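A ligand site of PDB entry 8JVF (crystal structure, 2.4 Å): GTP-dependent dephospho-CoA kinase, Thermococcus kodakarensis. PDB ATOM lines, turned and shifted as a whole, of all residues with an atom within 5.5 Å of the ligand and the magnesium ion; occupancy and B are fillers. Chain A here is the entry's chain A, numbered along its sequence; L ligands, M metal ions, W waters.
N of Glu 124 sits close to OD1 of Asp 67, at 3.2 Å. The side-chain hydroxyl of Thr 51 lies within hydrogen-bond range of the backbone carbonyl oxygen of Gly 47. O of Leu 65 sits at hydrogen-bond distance from N of Gly 47 (2.7 Å). O of Val 150 sits at hydrogen-bond distance from N of Val 23 (2.9 Å).
Residues that only touch the magnesium ion: Glu 124 (3.5 Å). Of the 27 residues printed, 1 comes within 4 Å of the magnesium ion. The nearest printed residue that does not touch the magnesium ion is Gly 47 (4.3 Å).
O3 of the ligand is bound to the magnesium ion (2.0 Å). O9 of the ligand binds the magnesium ion, 2.0 Å away. The magnesium ion is bound by water W1, at 2.3 Å. Water W2 binds the magnesium ion. Slightly farther from the magnesium ion lies O6 of the ligand (2.6 Å).
Water W5 bridges the backbone carbonyl oxygen of Val 46 (2.7 Å) and the backbone NH of Gly 144 (3.0 Å). Water W4 lies within hydrogen-bond range of an oxygen (O5) of the ligand (2.7 Å) and the side-chain amino group of Lys 69 (3.1 Å).
Residues that only touch the ligand: Ile 27, Pro 30, Gly 47, Tyr 66, Gly 144, Gln 145, Pro 146 and Val 150. 19 residues have an atom within 4 Å of the ligand: Gly 25, Ile 27, Pro 30, Tyr 31, Gly 47, Asp 48, Val 49, Val 50, Tyr 66, Asp 67, Lys 69, Glu 124, Gly 144, Gln 145, Pro 146, Asp 147, Glu 148, Gly 149 and Val 150. The nearest printed residue that does not touch the ligand is Val 46 (4.1 Å).
The side-chain carboxylate (OE2) of Glu 124 sits close to an oxygen (O3) of the ligand (2.5 Å). O2 of the ligand is in salt-bridge range of NZ of Lys 69, 2.6 Å away. N of Asp 48 lies within hydrogen-bond range of O1 of the ligand (3.1 Å). O1 of the ligand sits close to OD2 of Asp 48 (2.6 Å). A nitrogen (N3) of the ligand is in hydrogen-bond range of the backbone carbonyl oxygen (O) of Gly 25 (2.7 Å). OH of Tyr 31 is in hydrogen-bond range of N2 of the ligand (2.8 Å). N of Asp 147 sits at hydrogen-bond distance from O13 of the ligand. O of Asp 147 lies within hydrogen-bond range of N4 of the ligand (3.2 Å). The backbone NH of Val 49 lies within hydrogen-bond range of an oxygen (O8) of the ligand, 2.9 Å away. O1 of the ligand lies within hydrogen-bond range of N of Asp 67. The side-chain carboxylate (OD2) of Asp 67 lies close to an oxygen (O2) of the ligand, at 2.9 Å. The backbone NH (N) of Val 50 lies within hydrogen-bond range of an oxygen (O8) of the ligand (3.1 Å). A nitrogen (N5) of the ligand lies within hydrogen-bond range of the backbone NH of Gly 149 (3.3 Å). O of Glu 148 sits at hydrogen-bond distance from N4 of the ligand, at 3.4 Å.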
ATOM      1  N   VAL A  23       4.988  22.788  34.664  1.00  0.00           N
ATOM      2  CA  VAL A  23       6.334  23.117  34.206  1.00  0.00           C
ATOM      3  C   VAL A  23       6.229  24.262  33.205  1.00  0.00           C
ATOM      4  O   VAL A  23       5.575  24.136  32.170  1.00  0.00           O
ATOM      5  CB  VAL A  23       7.011  21.881  33.586  1.00  0.00           C
ATOM      6  CG1 VAL A  23       8.463  22.138  33.237  1.00  0.00           C
ATOM      7  CG2 VAL A  23       6.876  20.663  34.480  1.00  0.00           C
ATOM      8  N   ARG A  24       6.867  25.390  33.538  1.00  0.00           N
ATOM      9  CA  ARG A  24       6.649  26.641  32.836  1.00  0.00           C
ATOM     10  C   ARG A  24       7.716  26.813  31.761  1.00  0.00           C
ATOM     11  O   ARG A  24       8.784  26.213  31.843  1.00  0.00           O
ATOM     12  CB  ARG A  24       6.696  27.818  33.803  1.00  0.00           C
ATOM     13  CG  ARG A  24       5.708  27.730  34.956  1.00  0.00           C
ATOM     14  CD  ARG A  24       5.852  28.911  35.900  1.00  0.00           C
ATOM     15  NE  ARG A  24       4.599  29.232  36.575  1.00  0.00           N
ATOM     16  CZ  ARG A  24       3.547  29.798  36.004  1.00  0.00           C
ATOM     17  NH1 ARG A  24       3.623  30.224  34.753  1.00  0.00           N
ATOM     18  NH2 ARG A  24       2.414  29.927  36.671  1.00  0.00           N
ATOM     19  N   GLY A  25       7.450  27.703  30.803  1.00  0.00           N
ATOM     20  CA  GLY A  25       8.386  27.977  29.733  1.00  0.00           C
ATOM     21  C   GLY A  25       7.688  28.086  28.384  1.00  0.00           C
ATOM     22  O   GLY A  25       6.625  27.508  28.168  1.00  0.00           O
ATOM     23  N   PRO A  26       8.274  28.821  27.414  1.00  0.00           N
ATOM     24  CA  PRO A  26       7.753  28.825  26.042  1.00  0.00           C
ATOM     25  C   PRO A  26       7.935  27.458  25.399  1.00  0.00           C
ATOM     26  O   PRO A  26       8.897  26.753  25.692  1.00  0.00           O
ATOM     27  CB  PRO A  26       8.604  29.901  25.350  1.00  0.00           C
ATOM     28  CG  PRO A  26       9.923  29.888  26.109  1.00  0.00           C
ATOM     29  CD  PRO A  26       9.554  29.540  27.543  1.00  0.00           C
ATOM     30  N   ILE A  27       6.950  27.039  24.594  1.00  0.00           N
ATOM     31  CA  ILE A  27       7.052  25.831  23.805  1.00  0.00           C
ATOM     32  C   ILE A  27       8.370  25.889  23.015  1.00  0.00           C
ATOM     33  O   ILE A  27       8.639  26.881  22.362  1.00  0.00           O
ATOM     34  CB  ILE A  27       5.833  25.674  22.878  1.00  0.00           C
ATOM     35  CG1 ILE A  27       4.522  25.598  23.667  1.00  0.00           C
ATOM     36  CG2 ILE A  27       5.979  24.475  21.963  1.00  0.00           C
ATOM     37  CD1 ILE A  27       3.280  25.607  22.802  1.00  0.00           C
ATOM     38  N   PRO A  28       9.197  24.820  22.985  1.00  0.00           N
ATOM     39  CA  PRO A  28       8.886  23.545  23.646  1.00  0.00           C
ATOM     40  C   PRO A  28       9.769  23.169  24.829  1.00  0.00           C
ATOM     41  O   PRO A  28      10.012  21.998  25.088  1.00  0.00           O
ATOM     42  CB  PRO A  28       9.183  22.577  22.489  1.00  0.00           C
ATOM     43  CG  PRO A  28      10.449  23.162  21.870  1.00  0.00           C
ATOM     44  CD  PRO A  28      10.300  24.660  22.027  1.00  0.00           C
ATOM     45  N   GLU A  29      10.203  24.187  25.588  1.00  0.00           N
ATOM     46  CA  GLU A  29      11.284  24.025  26.542  1.00  0.00           C
ATOM     47  C   GLU A  29      10.862  23.075  27.655  1.00  0.00           C
ATOM     48  O   GLU A  29      11.640  22.216  28.066  1.00  0.00           O
ATOM     49  CB  GLU A  29      11.730  25.407  27.049  1.00  0.00           C
ATOM     50  CG  GLU A  29      12.211  26.315  25.923  1.00  0.00           C
ATOM     51  CD  GLU A  29      12.877  27.617  26.323  1.00  0.00           C
ATOM     52  OE1 GLU A  29      13.151  27.800  27.532  1.00  0.00           O
ATOM     53  OE2 GLU A  29      13.130  28.460  25.426  1.00  0.00           O
ATOM     54  N   PRO A  30       9.598  23.127  28.121  1.00  0.00           N
ATOM     55  CA  PRO A  30       9.133  22.202  29.164  1.00  0.00           C
ATOM     56  C   PRO A  30       9.174  20.723  28.779  1.00  0.00           C
ATOM     57  O   PRO A  30       9.346  19.865  29.633  1.00  0.00           O
ATOM     58  CB  PRO A  30       7.670  22.637  29.395  1.00  0.00           C
ATOM     59  CG  PRO A  30       7.631  24.083  28.946  1.00  0.00           C
ATOM     60  CD  PRO A  30       8.583  24.129  27.774  1.00  0.00           C
ATOM     61  N   TYR A  31       8.974  20.448  27.482  1.00  0.00           N
ATOM     62  CA  TYR A  31       9.039  19.100  26.965  1.00  0.00           C
ATOM     63  C   TYR A  31      10.485  18.614  27.028  1.00  0.00           C
ATOM     64  O   TYR A  31      10.749  17.455  27.341  1.00  0.00           O
ATOM     65  CB  TYR A  31       8.443  19.027  25.557  1.00  0.00           C
ATOM     66  CG  TYR A  31       6.986  19.423  25.490  1.00  0.00           C
ATOM     67  CD1 TYR A  31       5.979  18.511  25.758  1.00  0.00           C
ATOM     68  CD2 TYR A  31       6.615  20.754  25.305  1.00  0.00           C
ATOM     69  CE1 TYR A  31       4.652  18.885  25.828  1.00  0.00           C
ATOM     70  CE2 TYR A  31       5.279  21.140  25.326  1.00  0.00           C
ATOM     71  CZ  TYR A  31       4.301  20.207  25.593  1.00  0.00           C
ATOM     72  OH  TYR A  31       2.979  20.575  25.633  1.00  0.00           O
ATOM     73  N   VAL A  46      -2.871  14.594  26.780  1.00  0.00           N
ATOM     74  CA  VAL A  46      -4.168  15.206  26.532  1.00  0.00           C
ATOM     75  C   VAL A  46      -3.941  16.551  25.844  1.00  0.00           C
ATOM     76  O   VAL A  46      -3.344  17.466  26.418  1.00  0.00           O
ATOM     77  CB  VAL A  46      -4.955  15.373  27.856  1.00  0.00           C
ATOM     78  CG1 VAL A  46      -6.287  16.078  27.628  1.00  0.00           C
ATOM     79  CG2 VAL A  46      -5.158  14.045  28.568  1.00  0.00           C
ATOM     80  N   GLY A  47      -4.392  16.651  24.592  1.00  0.00           N
ATOM     81  CA  GLY A  47      -4.356  17.892  23.836  1.00  0.00           C
ATOM     82  C   GLY A  47      -3.483  17.759  22.583  1.00  0.00           C
ATOM     83  O   GLY A  47      -2.497  17.021  22.589  1.00  0.00           O
ATOM     84  N   ASP A  48      -3.829  18.533  21.553  1.00  0.00           N
ATOM     85  CA  ASP A  48      -3.139  18.508  20.282  1.00  0.00           C
ATOM     86  C   ASP A  48      -1.708  19.032  20.425  1.00  0.00           C
ATOM     87  O   ASP A  48      -0.795  18.512  19.789  1.00  0.00           O
ATOM     88  CB  ASP A  48      -3.874  19.337  19.233  1.00  0.00           C
ATOM     89  CG  ASP A  48      -4.868  18.557  18.387  1.00  0.00           C
ATOM     90  OD1 ASP A  48      -4.412  17.805  17.514  1.00  0.00           O
ATOM     91  OD2 ASP A  48      -6.094  18.783  18.565  1.00  0.00           O
ATOM     92  N   VAL A  49      -1.553  20.122  21.184  1.00  0.00           N
ATOM     93  CA  VAL A  49      -0.264  20.777  21.335  1.00  0.00           C
ATOM     94  C   VAL A  49       0.642  19.893  22.176  1.00  0.00           C
ATOM     95  O   VAL A  49       1.757  19.566  21.784  1.00  0.00           O
ATOM     96  CB  VAL A  49      -0.414  22.194  21.917  1.00  0.00           C
ATOM     97  CG1 VAL A  49       0.932  22.885  22.117  1.00  0.00           C
ATOM     98  CG2 VAL A  49      -1.325  23.067  21.064  1.00  0.00           C
ATOM     99  N   VAL A  50       0.097  19.339  23.266  1.00  0.00           N
ATOM    100  CA  VAL A  50       0.848  18.460  24.147  1.00  0.00           C
ATOM    101  C   VAL A  50       1.289  17.222  23.368  1.00  0.00           C
ATOM    102  O   VAL A  50       2.477  16.901  23.336  1.00  0.00           O
ATOM    103  CB  VAL A  50       0.018  18.098  25.385  1.00  0.00           C
ATOM    104  CG1 VAL A  50       0.737  17.088  26.276  1.00  0.00           C
ATOM    105  CG2 VAL A  50      -0.371  19.330  26.187  1.00  0.00           C
ATOM    106  N   THR A  51       0.332  16.585  22.686  1.00  0.00           N
ATOM    107  CA  THR A  51       0.615  15.363  21.939  1.00  0.00           C
ATOM    108  C   THR A  51       1.725  15.606  20.927  1.00  0.00           C
ATOM    109  O   THR A  51       2.704  14.870  20.893  1.00  0.00           O
ATOM    110  CB  THR A  51      -0.650  14.819  21.259  1.00  0.00           C
ATOM    111  OG1 THR A  51      -1.610  14.511  22.272  1.00  0.00           O
ATOM    112  CG2 THR A  51      -0.376  13.593  20.419  1.00  0.00           C
ATOM    113  N   LEU A  65      -5.092  11.731  23.615  1.00  0.00           N
ATOM    114  CA  LEU A  65      -6.436  12.246  23.421  1.00  0.00           C
ATOM    115  C   LEU A  65      -6.352  13.670  22.896  1.00  0.00           C
ATOM    116  O   LEU A  65      -5.838  14.544  23.580  1.00  0.00           O
ATOM    117  CB  LEU A  65      -7.195  12.293  24.761  1.00  0.00           C
ATOM    118  CG  LEU A  65      -7.420  10.969  25.461  1.00  0.00           C
ATOM    119  CD1 LEU A  65      -6.319  10.700  26.473  1.00  0.00           C
ATOM    120  CD2 LEU A  65      -8.780  10.952  26.133  1.00  0.00           C
ATOM    121  N   TYR A  66      -7.063  13.948  21.802  1.00  0.00           N
ATOM    122  CA  TYR A  66      -7.069  15.298  21.271  1.00  0.00           C
ATOM    123  C   TYR A  66      -8.344  15.565  20.480  1.00  0.00           C
ATOM    124  O   TYR A  66      -9.052  14.648  20.040  1.00  0.00           O
ATOM    125  CB  TYR A  66      -5.800  15.564  20.466  1.00  0.00           C
ATOM    126  CG  TYR A  66      -5.396  14.509  19.467  1.00  0.00           C
ATOM    127  CD1 TYR A  66      -4.629  13.415  19.844  1.00  0.00           C
ATOM    128  CD2 TYR A  66      -5.676  14.670  18.123  1.00  0.00           C
ATOM    129  CE1 TYR A  66      -4.165  12.502  18.909  1.00  0.00           C
ATOM    130  CE2 TYR A  66      -5.258  13.741  17.183  1.00  0.00           C
ATOM    131  CZ  TYR A  66      -4.487  12.657  17.582  1.00  0.00           C
ATOM    132  OH  TYR A  66      -4.063  11.739  16.654  1.00  0.00           O
ATOM    133  N   ASP A  67      -8.645  16.860  20.356  1.00  0.00           N
ATOM    134  CA  ASP A  67      -9.820  17.333  19.651  1.00  0.00           C
ATOM    135  C   ASP A  67      -9.557  17.236  18.148  1.00  0.00           C
ATOM    136  O   ASP A  67      -8.476  17.568  17.673  1.00  0.00           O
ATOM    137  CB  ASP A  67     -10.149  18.770  20.071  1.00  0.00           C
ATOM    138  CG  ASP A  67     -10.636  18.891  21.511  1.00  0.00           C
ATOM    139  OD1 ASP A  67     -11.010  17.859  22.091  1.00  0.00           O
ATOM    140  OD2 ASP A  67     -10.648  20.024  22.022  1.00  0.00           O
ATOM    141  N   LYS A  69      -9.708  18.611  14.524  1.00  0.00           N
ATOM    142  CA  LYS A  69      -9.767  19.850  13.771  1.00  0.00           C
ATOM    143  C   LYS A  69      -9.282  19.577  12.340  1.00  0.00           C
ATOM    144  O   LYS A  69      -9.136  20.559  11.586  1.00  0.00           O
ATOM    145  CB  LYS A  69      -8.928  20.924  14.455  1.00  0.00           C
ATOM    146  CG  LYS A  69      -9.393  21.337  15.846  1.00  0.00           C
ATOM    147  CD  LYS A  69      -8.329  22.016  16.673  1.00  0.00           C
ATOM    148  CE  LYS A  69      -8.716  22.181  18.126  1.00  0.00           C
ATOM    149  NZ  LYS A  69      -7.540  22.493  18.970  1.00  0.00           N
ATOM    150  N   GLU A 124     -12.134  17.824  25.063  1.00  0.00           N
ATOM    151  CA  GLU A 124     -11.561  16.836  25.958  1.00  0.00           C
ATOM    152  C   GLU A 124     -10.959  17.554  27.162  1.00  0.00           C
ATOM    153  O   GLU A 124      -9.955  17.132  27.721  1.00  0.00           O
ATOM    154  CB  GLU A 124     -10.535  15.998  25.184  1.00  0.00           C
ATOM    155  CG  GLU A 124      -9.117  16.544  25.198  1.00  0.00           C
ATOM    156  CD  GLU A 124      -8.894  17.816  24.388  1.00  0.00           C
ATOM    157  OE1 GLU A 124      -9.484  18.855  24.755  1.00  0.00           O
ATOM    158  OE2 GLU A 124      -8.096  17.772  23.426  1.00  0.00           O
ATOM    159  N   GLY A 144      -2.126  20.510  28.991  1.00  0.00           N
ATOM    160  CA  GLY A 144      -1.613  21.848  28.778  1.00  0.00           C
ATOM    161  C   GLY A 144      -2.346  22.887  29.641  1.00  0.00           C
ATOM    162  O   GLY A 144      -3.573  22.916  29.680  1.00  0.00           O
ATOM    163  N   GLN A 145      -1.565  23.728  30.318  1.00  0.00           N
ATOM    164  CA  GLN A 145      -2.105  24.860  31.065  1.00  0.00           C
ATOM    165  C   GLN A 145      -2.044  26.104  30.180  1.00  0.00           C
ATOM    166  O   GLN A 145      -0.960  26.607  29.901  1.00  0.00           O
ATOM    167  CB  GLN A 145      -1.324  25.054  32.362  1.00  0.00           C
ATOM    168  CG  GLN A 145      -2.035  25.945  33.377  1.00  0.00           C
ATOM    169  CD  GLN A 145      -3.435  25.454  33.686  1.00  0.00           C
ATOM    170  OE1 GLN A 145      -4.423  26.137  33.409  1.00  0.00           O
ATOM    171  NE2 GLN A 145      -3.531  24.266  34.253  1.00  0.00           N
ATOM    172  N   PRO A 146      -3.179  26.564  29.628  1.00  0.00           N
ATOM    173  CA  PRO A 146      -3.171  27.632  28.624  1.00  0.00           C
ATOM    174  C   PRO A 146      -2.193  28.764  28.951  1.00  0.00           C
ATOM    175  O   PRO A 146      -2.269  29.362  30.021  1.00  0.00           O
ATOM    176  CB  PRO A 146      -4.634  28.114  28.629  1.00  0.00           C
ATOM    177  CG  PRO A 146      -5.426  26.882  28.999  1.00  0.00           C
ATOM    178  CD  PRO A 146      -4.546  26.124  29.967  1.00  0.00           C
ATOM    179  N   ASP A 147      -1.215  28.947  28.063  1.00  0.00           N
ATOM    180  CA  ASP A 147      -0.320  30.086  28.072  1.00  0.00           C
ATOM    181  C   ASP A 147       0.761  29.892  29.122  1.00  0.00           C
ATOM    182  O   ASP A 147       1.856  30.435  28.991  1.00  0.00           O
ATOM    183  CB  ASP A 147      -1.079  31.410  28.233  1.00  0.00           C
ATOM    184  CG  ASP A 147      -1.945  31.773  27.029  1.00  0.00           C
ATOM    185  OD1 ASP A 147      -2.079  30.920  26.132  1.00  0.00           O
ATOM    186  OD2 ASP A 147      -2.476  32.901  26.997  1.00  0.00           O
ATOM    187  N   GLU A 148       0.515  28.981  30.071  1.00  0.00           N
ATOM    188  CA  GLU A 148       1.311  28.879  31.287  1.00  0.00           C
ATOM    189  C   GLU A 148       2.374  27.779  31.147  1.00  0.00           C
ATOM    190  O   GLU A 148       3.531  28.015  31.474  1.00  0.00           O
ATOM    191  CB  GLU A 148       0.408  28.627  32.464  1.00  0.00           C
ATOM    192  N   GLY A 149       1.963  26.583  30.709  1.00  0.00           N
ATOM    193  CA  GLY A 149       2.903  25.489  30.511  1.00  0.00           C
ATOM    194  C   GLY A 149       2.231  24.113  30.465  1.00  0.00           C
ATOM    195  O   GLY A 149       1.075  23.991  30.074  1.00  0.00           O
ATOM    196  N   VAL A 150       2.976  23.088  30.911  1.00  0.00           N
ATOM    197  CA  VAL A 150       2.546  21.707  30.820  1.00  0.00           C
ATOM    198  C   VAL A 150       2.416  21.137  32.230  1.00  0.00           C
ATOM    199  O   VAL A 150       3.383  21.097  32.980  1.00  0.00           O
ATOM    200  CB  VAL A 150       3.537  20.862  30.003  1.00  0.00           C
ATOM    201  CG1 VAL A 150       3.070  19.421  29.851  1.00  0.00           C
ATOM    202  CG2 VAL A 150       3.828  21.473  28.641  1.00  0.00           C
HETATM  203  P1  LIG L   1      -7.072  20.371  21.805  1.00  0.00           P
HETATM  204  O1  LIG L   1      -6.860  19.082  21.043  1.00  0.00           O
HETATM  205  O2  LIG L   1      -8.130  21.251  21.185  1.00  0.00           O
HETATM  206  O3  LIG L   1      -7.280  20.160  23.289  1.00  0.00           O
HETATM  207  O4  LIG L   1      -5.691  21.182  21.721  1.00  0.00           O
HETATM  208  P2  LIG L   1      -5.379  22.678  22.214  1.00  0.00           P
HETATM  209  O5  LIG L   1      -5.175  23.499  20.986  1.00  0.00           O
HETATM  210  O6  LIG L   1      -6.402  23.085  23.221  1.00  0.00           O
HETATM  211  O7  LIG L   1      -3.992  22.465  22.979  1.00  0.00           O
HETATM  212  P3  LIG L   1      -3.634  21.571  24.256  1.00  0.00           P
HETATM  213  O8  LIG L   1      -2.710  20.490  23.796  1.00  0.00           O
HETATM  214  O9  LIG L   1      -4.896  21.222  24.970  1.00  0.00           O
HETATM  215  O10 LIG L   1      -2.802  22.633  25.120  1.00  0.00           O
HETATM  216  C1  LIG L   1      -3.532  23.710  25.755  1.00  0.00           C
HETATM  217  C2  LIG L   1      -2.622  24.898  25.944  1.00  0.00           C
HETATM  218  O11 LIG L   1      -1.521  24.549  26.823  1.00  0.00           O
HETATM  219  C3  LIG L   1      -1.894  25.406  24.699  1.00  0.00           C
HETATM  220  O12 LIG L   1      -2.754  26.207  23.890  1.00  0.00           O
HETATM  221  C4  LIG L   1      -0.761  26.229  25.328  1.00  0.00           C
HETATM  222  O13 LIG L   1      -1.138  27.563  25.558  1.00  0.00           O
HETATM  223  C5  LIG L   1      -0.492  25.491  26.641  1.00  0.00           C
HETATM  224  N1  LIG L   1       0.801  24.820  26.638  1.00  0.00           N
HETATM  225  C6  LIG L   1       1.066  23.560  26.157  1.00  0.00           C
HETATM  226  N2  LIG L   1       2.345  23.266  26.176  1.00  0.00           N
HETATM  227  C7  LIG L   1       2.956  24.421  26.662  1.00  0.00           C
HETATM  228  C8  LIG L   1       4.342  24.708  26.880  1.00  0.00           C
HETATM  229  O14 LIG L   1       5.324  23.991  26.677  1.00  0.00           O
HETATM  230  N3  LIG L   1       4.520  26.006  27.377  1.00  0.00           N
HETATM  231  C9  LIG L   1       3.512  26.912  27.615  1.00  0.00           C
HETATM  232  N4  LIG L   1       3.886  28.113  28.081  1.00  0.00           N
HETATM  233  N5  LIG L   1       2.224  26.649  27.397  1.00  0.00           N
HETATM  234  C10 LIG L   1       2.017  25.389  26.944  1.00  0.00           C
HETATM  235 MG    MG M   1      -6.901  21.184  24.946  1.00  0.00          MG
HETATM  236  O   HOH W   1      -6.953  23.293  25.853  1.00  0.00           O
HETATM  237  O   HOH W   2      -8.697  22.530  23.823  1.00  0.00           O
HETATM  238  O   HOH W   3      -6.831  25.555  24.648  1.00  0.00           O
HETATM  239  O   HOH W   4      -4.578  23.013  18.410  1.00  0.00           O
HETATM  240  O   HOH W   5      -4.364  19.864  27.115  1.00  0.00           O
